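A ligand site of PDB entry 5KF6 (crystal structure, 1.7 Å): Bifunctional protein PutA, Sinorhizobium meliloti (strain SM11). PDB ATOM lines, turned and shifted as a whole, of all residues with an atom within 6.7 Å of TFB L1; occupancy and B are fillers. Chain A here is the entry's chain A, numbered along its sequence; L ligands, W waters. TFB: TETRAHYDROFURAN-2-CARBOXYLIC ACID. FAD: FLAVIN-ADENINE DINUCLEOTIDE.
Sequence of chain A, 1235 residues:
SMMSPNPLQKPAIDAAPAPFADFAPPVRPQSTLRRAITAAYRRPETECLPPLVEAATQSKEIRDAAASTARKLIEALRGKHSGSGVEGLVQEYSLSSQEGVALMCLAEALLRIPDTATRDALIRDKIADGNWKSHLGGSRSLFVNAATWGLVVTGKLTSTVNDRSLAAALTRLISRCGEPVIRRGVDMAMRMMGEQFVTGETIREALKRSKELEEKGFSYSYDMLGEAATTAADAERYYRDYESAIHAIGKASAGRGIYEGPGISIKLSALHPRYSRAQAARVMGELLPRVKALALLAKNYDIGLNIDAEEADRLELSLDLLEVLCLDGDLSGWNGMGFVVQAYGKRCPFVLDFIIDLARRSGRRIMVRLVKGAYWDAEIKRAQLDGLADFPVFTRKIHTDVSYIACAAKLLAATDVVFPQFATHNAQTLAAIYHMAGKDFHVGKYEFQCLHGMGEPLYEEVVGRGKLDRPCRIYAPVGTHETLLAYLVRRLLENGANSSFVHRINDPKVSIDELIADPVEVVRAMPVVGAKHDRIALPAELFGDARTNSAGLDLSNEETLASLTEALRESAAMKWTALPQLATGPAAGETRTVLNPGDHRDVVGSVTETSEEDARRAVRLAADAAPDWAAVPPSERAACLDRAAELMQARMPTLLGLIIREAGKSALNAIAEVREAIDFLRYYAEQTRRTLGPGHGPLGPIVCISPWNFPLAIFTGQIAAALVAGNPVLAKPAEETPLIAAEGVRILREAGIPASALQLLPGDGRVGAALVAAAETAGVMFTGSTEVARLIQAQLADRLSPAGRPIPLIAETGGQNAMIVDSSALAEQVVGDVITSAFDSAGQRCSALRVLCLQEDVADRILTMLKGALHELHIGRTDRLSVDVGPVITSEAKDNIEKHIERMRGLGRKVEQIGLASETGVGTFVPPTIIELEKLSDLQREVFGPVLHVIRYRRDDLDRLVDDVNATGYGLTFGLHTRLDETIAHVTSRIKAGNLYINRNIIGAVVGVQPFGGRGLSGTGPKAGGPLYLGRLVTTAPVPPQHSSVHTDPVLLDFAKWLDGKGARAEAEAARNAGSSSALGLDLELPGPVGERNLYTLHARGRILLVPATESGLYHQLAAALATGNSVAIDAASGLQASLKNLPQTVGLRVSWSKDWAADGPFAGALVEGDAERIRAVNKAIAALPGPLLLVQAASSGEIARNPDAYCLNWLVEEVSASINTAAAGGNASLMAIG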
ATOM      1  N   ASP A 223       0.397 -12.974   8.827  1.00  0.00           N
ATOM      2  CA  ASP A 223      -0.726 -12.728   9.719  1.00  0.00           C
ATOM      3  C   ASP A 223      -1.392 -14.059  10.051  1.00  0.00           C
ATOM      4  O   ASP A 223      -2.018 -14.671   9.174  1.00  0.00           O
ATOM      5  CB  ASP A 223      -1.730 -11.792   9.062  1.00  0.00           C
ATOM      6  CG  ASP A 223      -2.990 -11.648   9.885  1.00  0.00           C
ATOM      7  OD1 ASP A 223      -2.858 -11.494  11.117  1.00  0.00           O
ATOM      8  OD2 ASP A 223      -4.071 -11.692   9.301  1.00  0.00           O
ATOM      9  N   GLU A 227      -8.813 -12.179  15.165  1.00  0.00           N
ATOM     10  CA  GLU A 227      -9.196 -10.838  15.585  1.00  0.00           C
ATOM     11  C   GLU A 227     -10.397 -10.993  16.482  1.00  0.00           C
ATOM     12  O   GLU A 227     -11.068 -12.035  16.484  1.00  0.00           O
ATOM     13  CB  GLU A 227      -9.523  -9.946  14.378  1.00  0.00           C
ATOM     14  CG  GLU A 227     -10.824 -10.295  13.692  1.00  0.00           C
ATOM     15  CD  GLU A 227     -10.928  -9.715  12.287  1.00  0.00           C
ATOM     16  OE1 GLU A 227      -9.986  -9.910  11.481  1.00  0.00           O
ATOM     17  OE2 GLU A 227     -11.966  -9.074  11.984  1.00  0.00           O
ATOM     18  N   SER A 265       2.635  -9.720  11.600  1.00  0.00           N
ATOM     19  CA  SER A 265       1.636  -8.705  11.923  1.00  0.00           C
ATOM     20  C   SER A 265       0.679  -9.288  12.952  1.00  0.00           C
ATOM     21  O   SER A 265       0.384 -10.483  12.905  1.00  0.00           O
ATOM     22  CB  SER A 265       0.865  -8.239  10.675  1.00  0.00           C
ATOM     23  OG  SER A 265       1.715  -7.539   9.762  1.00  0.00           O
ATOM     24  N   LYS A 267      -2.962  -8.340  15.607  1.00  0.00           N
ATOM     25  CA  LYS A 267      -4.090  -7.463  15.914  1.00  0.00           C
ATOM     26  C   LYS A 267      -4.273  -7.450  17.413  1.00  0.00           C
ATOM     27  O   LYS A 267      -4.367  -8.517  18.040  1.00  0.00           O
ATOM     28  CB  LYS A 267      -5.368  -7.948  15.208  1.00  0.00           C
ATOM     29  CG  LYS A 267      -5.398  -7.663  13.739  1.00  0.00           C
ATOM     30  CD  LYS A 267      -6.708  -8.186  13.099  1.00  0.00           C
ATOM     31  CE  LYS A 267      -6.990  -7.508  11.745  1.00  0.00           C
ATOM     32  NZ  LYS A 267      -5.929  -7.754  10.743  1.00  0.00           N
ATOM     33  N   ASN A 306       4.545  -6.007  13.525  1.00  0.00           N
ATOM     34  CA  ASN A 306       3.701  -4.868  13.192  1.00  0.00           C
ATOM     35  C   ASN A 306       2.357  -4.962  13.900  1.00  0.00           C
ATOM     36  O   ASN A 306       1.713  -6.017  13.879  1.00  0.00           O
ATOM     37  CB  ASN A 306       3.430  -4.812  11.680  1.00  0.00           C
ATOM     38  CG  ASN A 306       2.332  -3.827  11.312  1.00  0.00           C
ATOM     39  OD1 ASN A 306       1.143  -4.194  11.188  1.00  0.00           O
ATOM     40  ND2 ASN A 306       2.713  -2.583  11.164  1.00  0.00           N
ATOM     41  N   ASP A 308      -1.335  -4.123  13.566  1.00  0.00           N
ATOM     42  CA  ASP A 308      -2.352  -3.726  12.595  1.00  0.00           C
ATOM     43  C   ASP A 308      -3.286  -2.681  13.206  1.00  0.00           C
ATOM     44  O   ASP A 308      -3.484  -2.638  14.429  1.00  0.00           O
ATOM     45  CB  ASP A 308      -3.199  -4.928  12.145  1.00  0.00           C
ATOM     46  CG  ASP A 308      -2.461  -5.883  11.238  1.00  0.00           C
ATOM     47  OD1 ASP A 308      -1.356  -5.586  10.745  1.00  0.00           O
ATOM     48  OD2 ASP A 308      -3.030  -6.967  10.988  1.00  0.00           O
ATOM     49  N   ALA A 309      -3.878  -1.835  12.358  1.00  0.00           N
ATOM     50  CA  ALA A 309      -4.817  -0.823  12.834  1.00  0.00           C
ATOM     51  C   ALA A 309      -6.249  -1.297  12.620  1.00  0.00           C
ATOM     52  O   ALA A 309      -6.560  -1.885  11.581  1.00  0.00           O
ATOM     53  CB  ALA A 309      -4.604   0.536  12.131  1.00  0.00           C
ATOM     54  N   VAL A 340       0.615   0.531  12.152  1.00  0.00           N
ATOM     55  CA  VAL A 340      -0.176   0.976  11.013  1.00  0.00           C
ATOM     56  C   VAL A 340      -0.872   2.287  11.350  1.00  0.00           C
ATOM     57  O   VAL A 340      -1.396   2.454  12.465  1.00  0.00           O
ATOM     58  CB  VAL A 340      -1.233  -0.084  10.648  1.00  0.00           C
ATOM     59  CG1 VAL A 340      -2.132   0.439   9.521  1.00  0.00           C
ATOM     60  CG2 VAL A 340      -0.571  -1.390  10.274  1.00  0.00           C
ATOM     61  N   ARG A 369       3.533   1.544   8.758  1.00  0.00           N
ATOM     62  CA  ARG A 369       2.785   1.149   7.574  1.00  0.00           C
ATOM     63  C   ARG A 369       1.668   2.158   7.322  1.00  0.00           C
ATOM     64  O   ARG A 369       0.728   2.272   8.127  1.00  0.00           O
ATOM     65  CB  ARG A 369       2.201  -0.255   7.716  1.00  0.00           C
ATOM     66  CG  ARG A 369       1.505  -0.708   6.430  1.00  0.00           C
ATOM     67  CD  ARG A 369       0.605  -1.921   6.724  1.00  0.00           C
ATOM     68  NE  ARG A 369       1.381  -3.101   7.104  1.00  0.00           N
ATOM     69  CZ  ARG A 369       0.882  -4.113   7.821  1.00  0.00           C
ATOM     70  NH1 ARG A 369      -0.372  -4.071   8.251  1.00  0.00           N
ATOM     71  NH2 ARG A 369       1.656  -5.157   8.104  1.00  0.00           N
ATOM     72  N   ALA A 374      -9.446  -0.253   6.211  1.00  0.00           N
ATOM     73  CA  ALA A 374     -10.172  -1.461   5.847  1.00  0.00           C
ATOM     74  C   ALA A 374     -11.587  -1.544   6.393  1.00  0.00           C
ATOM     75  O   ALA A 374     -12.312  -2.482   6.043  1.00  0.00           O
ATOM     76  CB  ALA A 374      -9.395  -2.713   6.308  1.00  0.00           C
ATOM     77  N   TYR A 375     -11.987  -0.592   7.230  1.00  0.00           N
ATOM     78  CA  TYR A 375     -13.247  -0.675   7.981  1.00  0.00           C
ATOM     79  C   TYR A 375     -14.207   0.451   7.632  1.00  0.00           C
ATOM     80  O   TYR A 375     -14.996   0.859   8.488  1.00  0.00           O
ATOM     81  CB  TYR A 375     -12.979  -0.674   9.494  1.00  0.00           C
ATOM     82  CG  TYR A 375     -12.004  -1.746   9.924  1.00  0.00           C
ATOM     83  CD1 TYR A 375     -10.631  -1.496   9.912  1.00  0.00           C
ATOM     84  CD2 TYR A 375     -12.442  -2.999  10.299  1.00  0.00           C
ATOM     85  CE1 TYR A 375      -9.715  -2.486  10.277  1.00  0.00           C
ATOM     86  CE2 TYR A 375     -11.559  -3.995  10.666  1.00  0.00           C
ATOM     87  CZ  TYR A 375     -10.190  -3.737  10.657  1.00  0.00           C
ATOM     88  OH  TYR A 375      -9.328  -4.733  11.020  1.00  0.00           O
ATOM     89  N   LEU A 451      -1.110  -6.850  -0.418  1.00  0.00           N
ATOM     90  CA  LEU A 451      -1.776  -8.019   0.158  1.00  0.00           C
ATOM     91  C   LEU A 451      -1.585  -9.219  -0.756  1.00  0.00           C
ATOM     92  O   LEU A 451      -1.622  -9.099  -1.977  1.00  0.00           O
ATOM     93  CB  LEU A 451      -3.269  -7.720   0.364  1.00  0.00           C
ATOM     94  CG  LEU A 451      -3.621  -6.641   1.418  1.00  0.00           C
ATOM     95  CD1 LEU A 451      -5.109  -6.350   1.468  1.00  0.00           C
ATOM     96  CD2 LEU A 451      -3.137  -7.031   2.819  1.00  0.00           C
ATOM     97  N   TYR A 475       1.768  -8.882   2.597  1.00  0.00           N
ATOM     98  CA  TYR A 475       1.008  -9.239   3.790  1.00  0.00           C
ATOM     99  C   TYR A 475       0.347 -10.589   3.544  1.00  0.00           C
ATOM    100  O   TYR A 475      -0.508 -10.711   2.662  1.00  0.00           O
ATOM    101  CB  TYR A 475      -0.033  -8.173   4.103  1.00  0.00           C
ATOM    102  CG  TYR A 475      -0.768  -8.331   5.427  1.00  0.00           C
ATOM    103  CD1 TYR A 475      -1.846  -9.211   5.552  1.00  0.00           C
ATOM    104  CD2 TYR A 475      -0.411  -7.576   6.545  1.00  0.00           C
ATOM    105  CE1 TYR A 475      -2.534  -9.332   6.768  1.00  0.00           C
ATOM    106  CE2 TYR A 475      -1.084  -7.698   7.753  1.00  0.00           C
ATOM    107  CZ  TYR A 475      -2.141  -8.587   7.866  1.00  0.00           C
ATOM    108  OH  TYR A 475      -2.821  -8.710   9.061  1.00  0.00           O
ATOM    109  N   ALA A 486     -13.820 -13.284   8.204  1.00  0.00           N
ATOM    110  CA  ALA A 486     -13.926 -11.831   8.305  1.00  0.00           C
ATOM    111  C   ALA A 486     -12.898 -11.133   7.414  1.00  0.00           C
ATOM    112  O   ALA A 486     -13.241 -10.254   6.605  1.00  0.00           O
ATOM    113  CB  ALA A 486     -13.760 -11.394   9.759  1.00  0.00           C
ATOM    114  N   TYR A 487     -11.629 -11.517   7.536  1.00  0.00           N
ATOM    115  CA  TYR A 487     -10.604 -10.953   6.688  1.00  0.00           C
ATOM    116  C   TYR A 487     -10.937 -11.118   5.205  1.00  0.00           C
ATOM    117  O   TYR A 487     -10.749 -10.194   4.405  1.00  0.00           O
ATOM    118  CB  TYR A 487      -9.270 -11.625   7.012  1.00  0.00           C
ATOM    119  CG  TYR A 487      -8.116 -11.209   6.148  1.00  0.00           C
ATOM    120  CD1 TYR A 487      -7.892 -11.809   4.929  1.00  0.00           C
ATOM    121  CD2 TYR A 487      -7.221 -10.222   6.573  1.00  0.00           C
ATOM    122  CE1 TYR A 487      -6.844 -11.453   4.142  1.00  0.00           C
ATOM    123  CE2 TYR A 487      -6.145  -9.851   5.786  1.00  0.00           C
ATOM    124  CZ  TYR A 487      -5.964 -10.486   4.567  1.00  0.00           C
ATOM    125  OH  TYR A 487      -4.918 -10.143   3.741  1.00  0.00           O
ATOM    126  N   ARG A 490     -13.679  -8.627   3.978  1.00  0.00           N
ATOM    127  CA  ARG A 490     -13.083  -7.302   3.806  1.00  0.00           C
ATOM    128  C   ARG A 490     -12.292  -7.218   2.516  1.00  0.00           C
ATOM    129  O   ARG A 490     -12.311  -6.185   1.832  1.00  0.00           O
ATOM    130  CB  ARG A 490     -12.199  -6.944   5.011  1.00  0.00           C
ATOM    131  CG  ARG A 490     -12.985  -6.538   6.263  1.00  0.00           C
ATOM    132  CD  ARG A 490     -12.121  -5.880   7.348  1.00  0.00           C
ATOM    133  NE  ARG A 490     -10.980  -6.714   7.732  1.00  0.00           N
ATOM    134  CZ  ARG A 490     -10.967  -7.541   8.775  1.00  0.00           C
ATOM    135  NH1 ARG A 490     -12.045  -7.639   9.554  1.00  0.00           N
ATOM    136  NH2 ARG A 490      -9.888  -8.266   9.039  1.00  0.00           N
ATOM    137  N   ARG A 491     -11.607  -8.305   2.127  1.00  0.00           N
ATOM    138  CA  ARG A 491     -10.890  -8.304   0.855  1.00  0.00           C
ATOM    139  C   ARG A 491     -11.847  -8.283  -0.327  1.00  0.00           C
ATOM    140  O   ARG A 491     -11.696  -7.483  -1.252  1.00  0.00           O
ATOM    141  CB  ARG A 491      -9.978  -9.519   0.753  1.00  0.00           C
ATOM    142  CG  ARG A 491      -8.983  -9.678   1.873  1.00  0.00           C
ATOM    143  CD  ARG A 491      -7.848  -8.669   1.781  1.00  0.00           C
ATOM    144  NE  ARG A 491      -8.237  -7.323   2.212  1.00  0.00           N
ATOM    145  CZ  ARG A 491      -8.458  -6.971   3.471  1.00  0.00           C
ATOM    146  NH1 ARG A 491      -8.375  -7.889   4.435  1.00  0.00           N
ATOM    147  NH2 ARG A 491      -8.776  -5.716   3.790  1.00  0.00           N
ATOM    148  N   GLU A 494     -13.491  -4.975  -0.788  1.00  0.00           N
ATOM    149  CA  GLU A 494     -12.480  -4.114  -1.394  1.00  0.00           C
ATOM    150  C   GLU A 494     -12.347  -4.383  -2.888  1.00  0.00           C
ATOM    151  O   GLU A 494     -12.289  -3.446  -3.697  1.00  0.00           O
ATOM    152  CB  GLU A 494     -11.146  -4.313  -0.644  1.00  0.00           C
ATOM    153  CG  GLU A 494      -9.909  -3.614  -1.198  1.00  0.00           C
ATOM    154  CD  GLU A 494      -8.630  -3.994  -0.423  1.00  0.00           C
ATOM    155  OE1 GLU A 494      -8.717  -4.774   0.555  1.00  0.00           O
ATOM    156  OE2 GLU A 494      -7.538  -3.518  -0.790  1.00  0.00           O
HETATM  157  OA  TFB L   1      -5.495  -5.165   8.197  1.00  0.00           O
HETATM  158  CA  TFB L   1      -6.394  -5.270   7.105  1.00  0.00           C
HETATM  159  C   TFB L   1      -7.445  -6.335   7.377  1.00  0.00           C
HETATM  160  OB  TFB L   1      -8.416  -6.483   6.562  1.00  0.00           O
HETATM  161  CB  TFB L   1      -5.601  -5.641   5.946  1.00  0.00           C
HETATM  162  CG  TFB L   1      -4.387  -6.242   6.474  1.00  0.00           C
HETATM  163  CD  TFB L   1      -4.347  -5.936   7.894  1.00  0.00           C
HETATM  164  OXT TFB L   1      -7.370  -7.070   8.427  1.00  0.00           O
HETATM  165  PA  FAD L   2      -7.792   2.165  -3.410  1.00  0.00           P
HETATM  166  O1A FAD L   2      -8.791   1.599  -4.459  1.00  0.00           O
HETATM  167  O2A FAD L   2      -6.908   3.224  -3.848  1.00  0.00           O
HETATM  168  O5B FAD L   2      -8.377   2.759  -2.174  1.00  0.00           O
HETATM  169  C5B FAD L   2      -9.494   2.116  -1.541  1.00  0.00           C
HETATM  170  C4B FAD L   2      -9.736   2.664  -0.149  1.00  0.00           C
HETATM  171  O4B FAD L   2     -10.364   3.905  -0.191  1.00  0.00           O
HETATM  172  C3B FAD L   2     -10.625   1.821   0.696  1.00  0.00           C
HETATM  173  O3B FAD L   2     -10.020   0.658   1.173  1.00  0.00           O
HETATM  174  C2B FAD L   2     -10.954   2.794   1.786  1.00  0.00           C
HETATM  175  O2B FAD L   2      -9.920   2.922   2.704  1.00  0.00           O
HETATM  176  C1B FAD L   2     -11.060   4.065   1.020  1.00  0.00           C
HETATM  177  N9A FAD L   2     -12.395   4.466   0.650  1.00  0.00           N
HETATM  178  C8A FAD L   2     -13.275   3.794  -0.190  1.00  0.00           C
HETATM  179  N7A FAD L   2     -14.399   4.517  -0.299  1.00  0.00           N
HETATM  180  C5A FAD L   2     -14.266   5.680   0.440  1.00  0.00           C
HETATM  181  C6A FAD L   2     -15.075   6.779   0.680  1.00  0.00           C
HETATM  182  N6A FAD L   2     -16.377   6.874   0.090  1.00  0.00           N
HETATM  183  N1A FAD L   2     -14.632   7.764   1.480  1.00  0.00           N
HETATM  184  C2A FAD L   2     -13.391   7.728   2.039  1.00  0.00           C
HETATM  185  N3A FAD L   2     -12.570   6.665   1.817  1.00  0.00           N
HETATM  186  C4A FAD L   2     -12.990   5.663   1.036  1.00  0.00           C
HETATM  187  N1  FAD L   2      -6.202  -1.257   6.612  1.00  0.00           N
HETATM  188  C2  FAD L   2      -6.517  -1.163   7.998  1.00  0.00           C
HETATM  189  O2  FAD L   2      -7.635  -0.535   8.357  1.00  0.00           O
HETATM  190  N3  FAD L   2      -5.685  -1.684   8.960  1.00  0.00           N
HETATM  191  C4  FAD L   2      -4.537  -2.339   8.585  1.00  0.00           C
HETATM  192  O4  FAD L   2      -3.732  -2.830   9.554  1.00  0.00           O
HETATM  193  C4X FAD L   2      -4.169  -2.500   7.169  1.00  0.00           C
HETATM  194  N5  FAD L   2      -3.015  -3.160   6.749  1.00  0.00           N
HETATM  195  C5X FAD L   2      -2.746  -3.235   5.372  1.00  0.00           C
HETATM  196  C6  FAD L   2      -1.593  -3.903   4.937  1.00  0.00           C
HETATM  197  C7  FAD L   2      -1.306  -3.987   3.582  1.00  0.00           C
HETATM  198  C7M FAD L   2      -0.045  -4.707   3.168  1.00  0.00           C
HETATM  199  C8  FAD L   2      -2.148  -3.403   2.634  1.00  0.00           C
HETATM  200  C8M FAD L   2      -1.863  -3.465   1.167  1.00  0.00           C
HETATM  201  C9  FAD L   2      -3.299  -2.731   3.059  1.00  0.00           C
HETATM  202  C9A FAD L   2      -3.588  -2.652   4.423  1.00  0.00           C
HETATM  203  N10 FAD L   2      -4.767  -1.974   4.857  1.00  0.00           N
HETATM  204  C10 FAD L   2      -5.063  -1.895   6.208  1.00  0.00           C
HETATM  205  C1' FAD L   2      -5.644  -1.280   3.871  1.00  0.00           C
HETATM  206  C2' FAD L   2      -6.913  -1.983   3.461  1.00  0.00           C
HETATM  207  O2' FAD L   2      -6.820  -3.296   3.845  1.00  0.00           O
HETATM  208  C3' FAD L   2      -7.019  -1.839   1.929  1.00  0.00           C
HETATM  209  O3' FAD L   2      -6.109  -2.746   1.404  1.00  0.00           O
HETATM  210  C4' FAD L   2      -6.742  -0.446   1.384  1.00  0.00           C
HETATM  211  O4' FAD L   2      -7.457   0.527   2.083  1.00  0.00           O
HETATM  212  C5' FAD L   2      -7.019  -0.299  -0.124  1.00  0.00           C
HETATM  213  O5' FAD L   2      -6.305   0.855  -0.564  1.00  0.00           O
HETATM  214  P   FAD L   2      -5.561   1.047  -1.983  1.00  0.00           P
HETATM  215  O1P FAD L   2      -4.528   2.215  -2.084  1.00  0.00           O
HETATM  216  O2P FAD L   2      -5.043  -0.386  -2.284  1.00  0.00           O
HETATM  217  O3P FAD L   2      -6.826   1.085  -3.007  1.00  0.00           O
HETATM  218  O   HOH W   1      -6.568  -4.480  10.632  1.00  0.00           O
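NZ of Lys 267 lies within salt-bridge range of OXT of TFB L1.
An oxygen (O3') of FAD L2 is in hydrogen-bond range of the side-chain carboxylate of Glu 494 (2.7 Å).
An oxygen (OB) of TFB L1 lies within salt-bridge range of the guanidinium group (NE) of Arg 490, at 2.8 Å.
NH1 of Arg 369 is in hydrogen-bond range of N5 of FAD L2, 3.2 Å away.
The backbone NH (N) of Ala 374 sits at hydrogen-bond distance from an oxygen (O2) of FAD L2.
An oxygen (OB) of TFB L1 is in salt-bridge range of the guanidinium group (NH1) of Arg 491, 2.6 Å away.
A nitrogen (N3) of FAD L2 sits at hydrogen-bond distance from the backbone carbonyl oxygen (O) of Ala 309 (2.8 Å).
An oxygen (O2') of FAD L2 sits at hydrogen-bond distance from the guanidinium group (NH2) of Arg 491 (3.1 Å).
An oxygen (O4) of FAD L2 sits at hydrogen-bond distance from the backbone NH (N) of Ala 309 (3.0 Å).
The side-chain carboxylate of Asp 223 sits close to the side-chain hydroxyl of Tyr 475 (3.2 Å).
The side-chain carboxylate (OD1) of Asp 308 sits close to the side-chain amide oxygen (OD1) of Asn 306.
NE of Arg 491 is in salt-bridge range of OE1 of Glu 494, 3.1 Å away.
OE2 of Glu 227 is in salt-bridge range of NH1 of Arg 490 (2.8 Å).
The side-chain carboxylate of Asp 308 lies within salt-bridge range of the side-chain amino group of Lys 267 (3.0 Å).
The guanidinium group (NH1) of Arg 491 sits close to the backbone carbonyl oxygen (O) of Tyr 487.
OD1 of Asp 308 lies within salt-bridge range of NH1 of Arg 369, at 3.1 Å.
OH of Tyr 475 is in hydrogen-bond range of OD2 of Asp 308.
OD2 of Asp 308 touches CD of TFB L1, 3.5 Å away.
CB of Ala 374 touches OB of TFB L1, at 3.9 Å.
CD2 of Leu 451 touches CG of TFB L1 (3.9 Å).
Tyr 475 touches TFB L1 (OH to CD, 3.4 Å).
Tyr 487 touches TFB L1.
Of the 18 residues printed, 8 come within 4 Å of TFB L1.
The nearest printed residue that does not touch TFB L1 is Tyr 375 (4.002 Å).
Water W1 lies within hydrogen-bond range of an oxygen (OA) of TFB L1, the backbone carbonyl oxygen of Ala 309, the side-chain hydroxyl of Tyr 375, the side-chain amino group of Lys 267 and a nitrogen (N3) of FAD L2.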
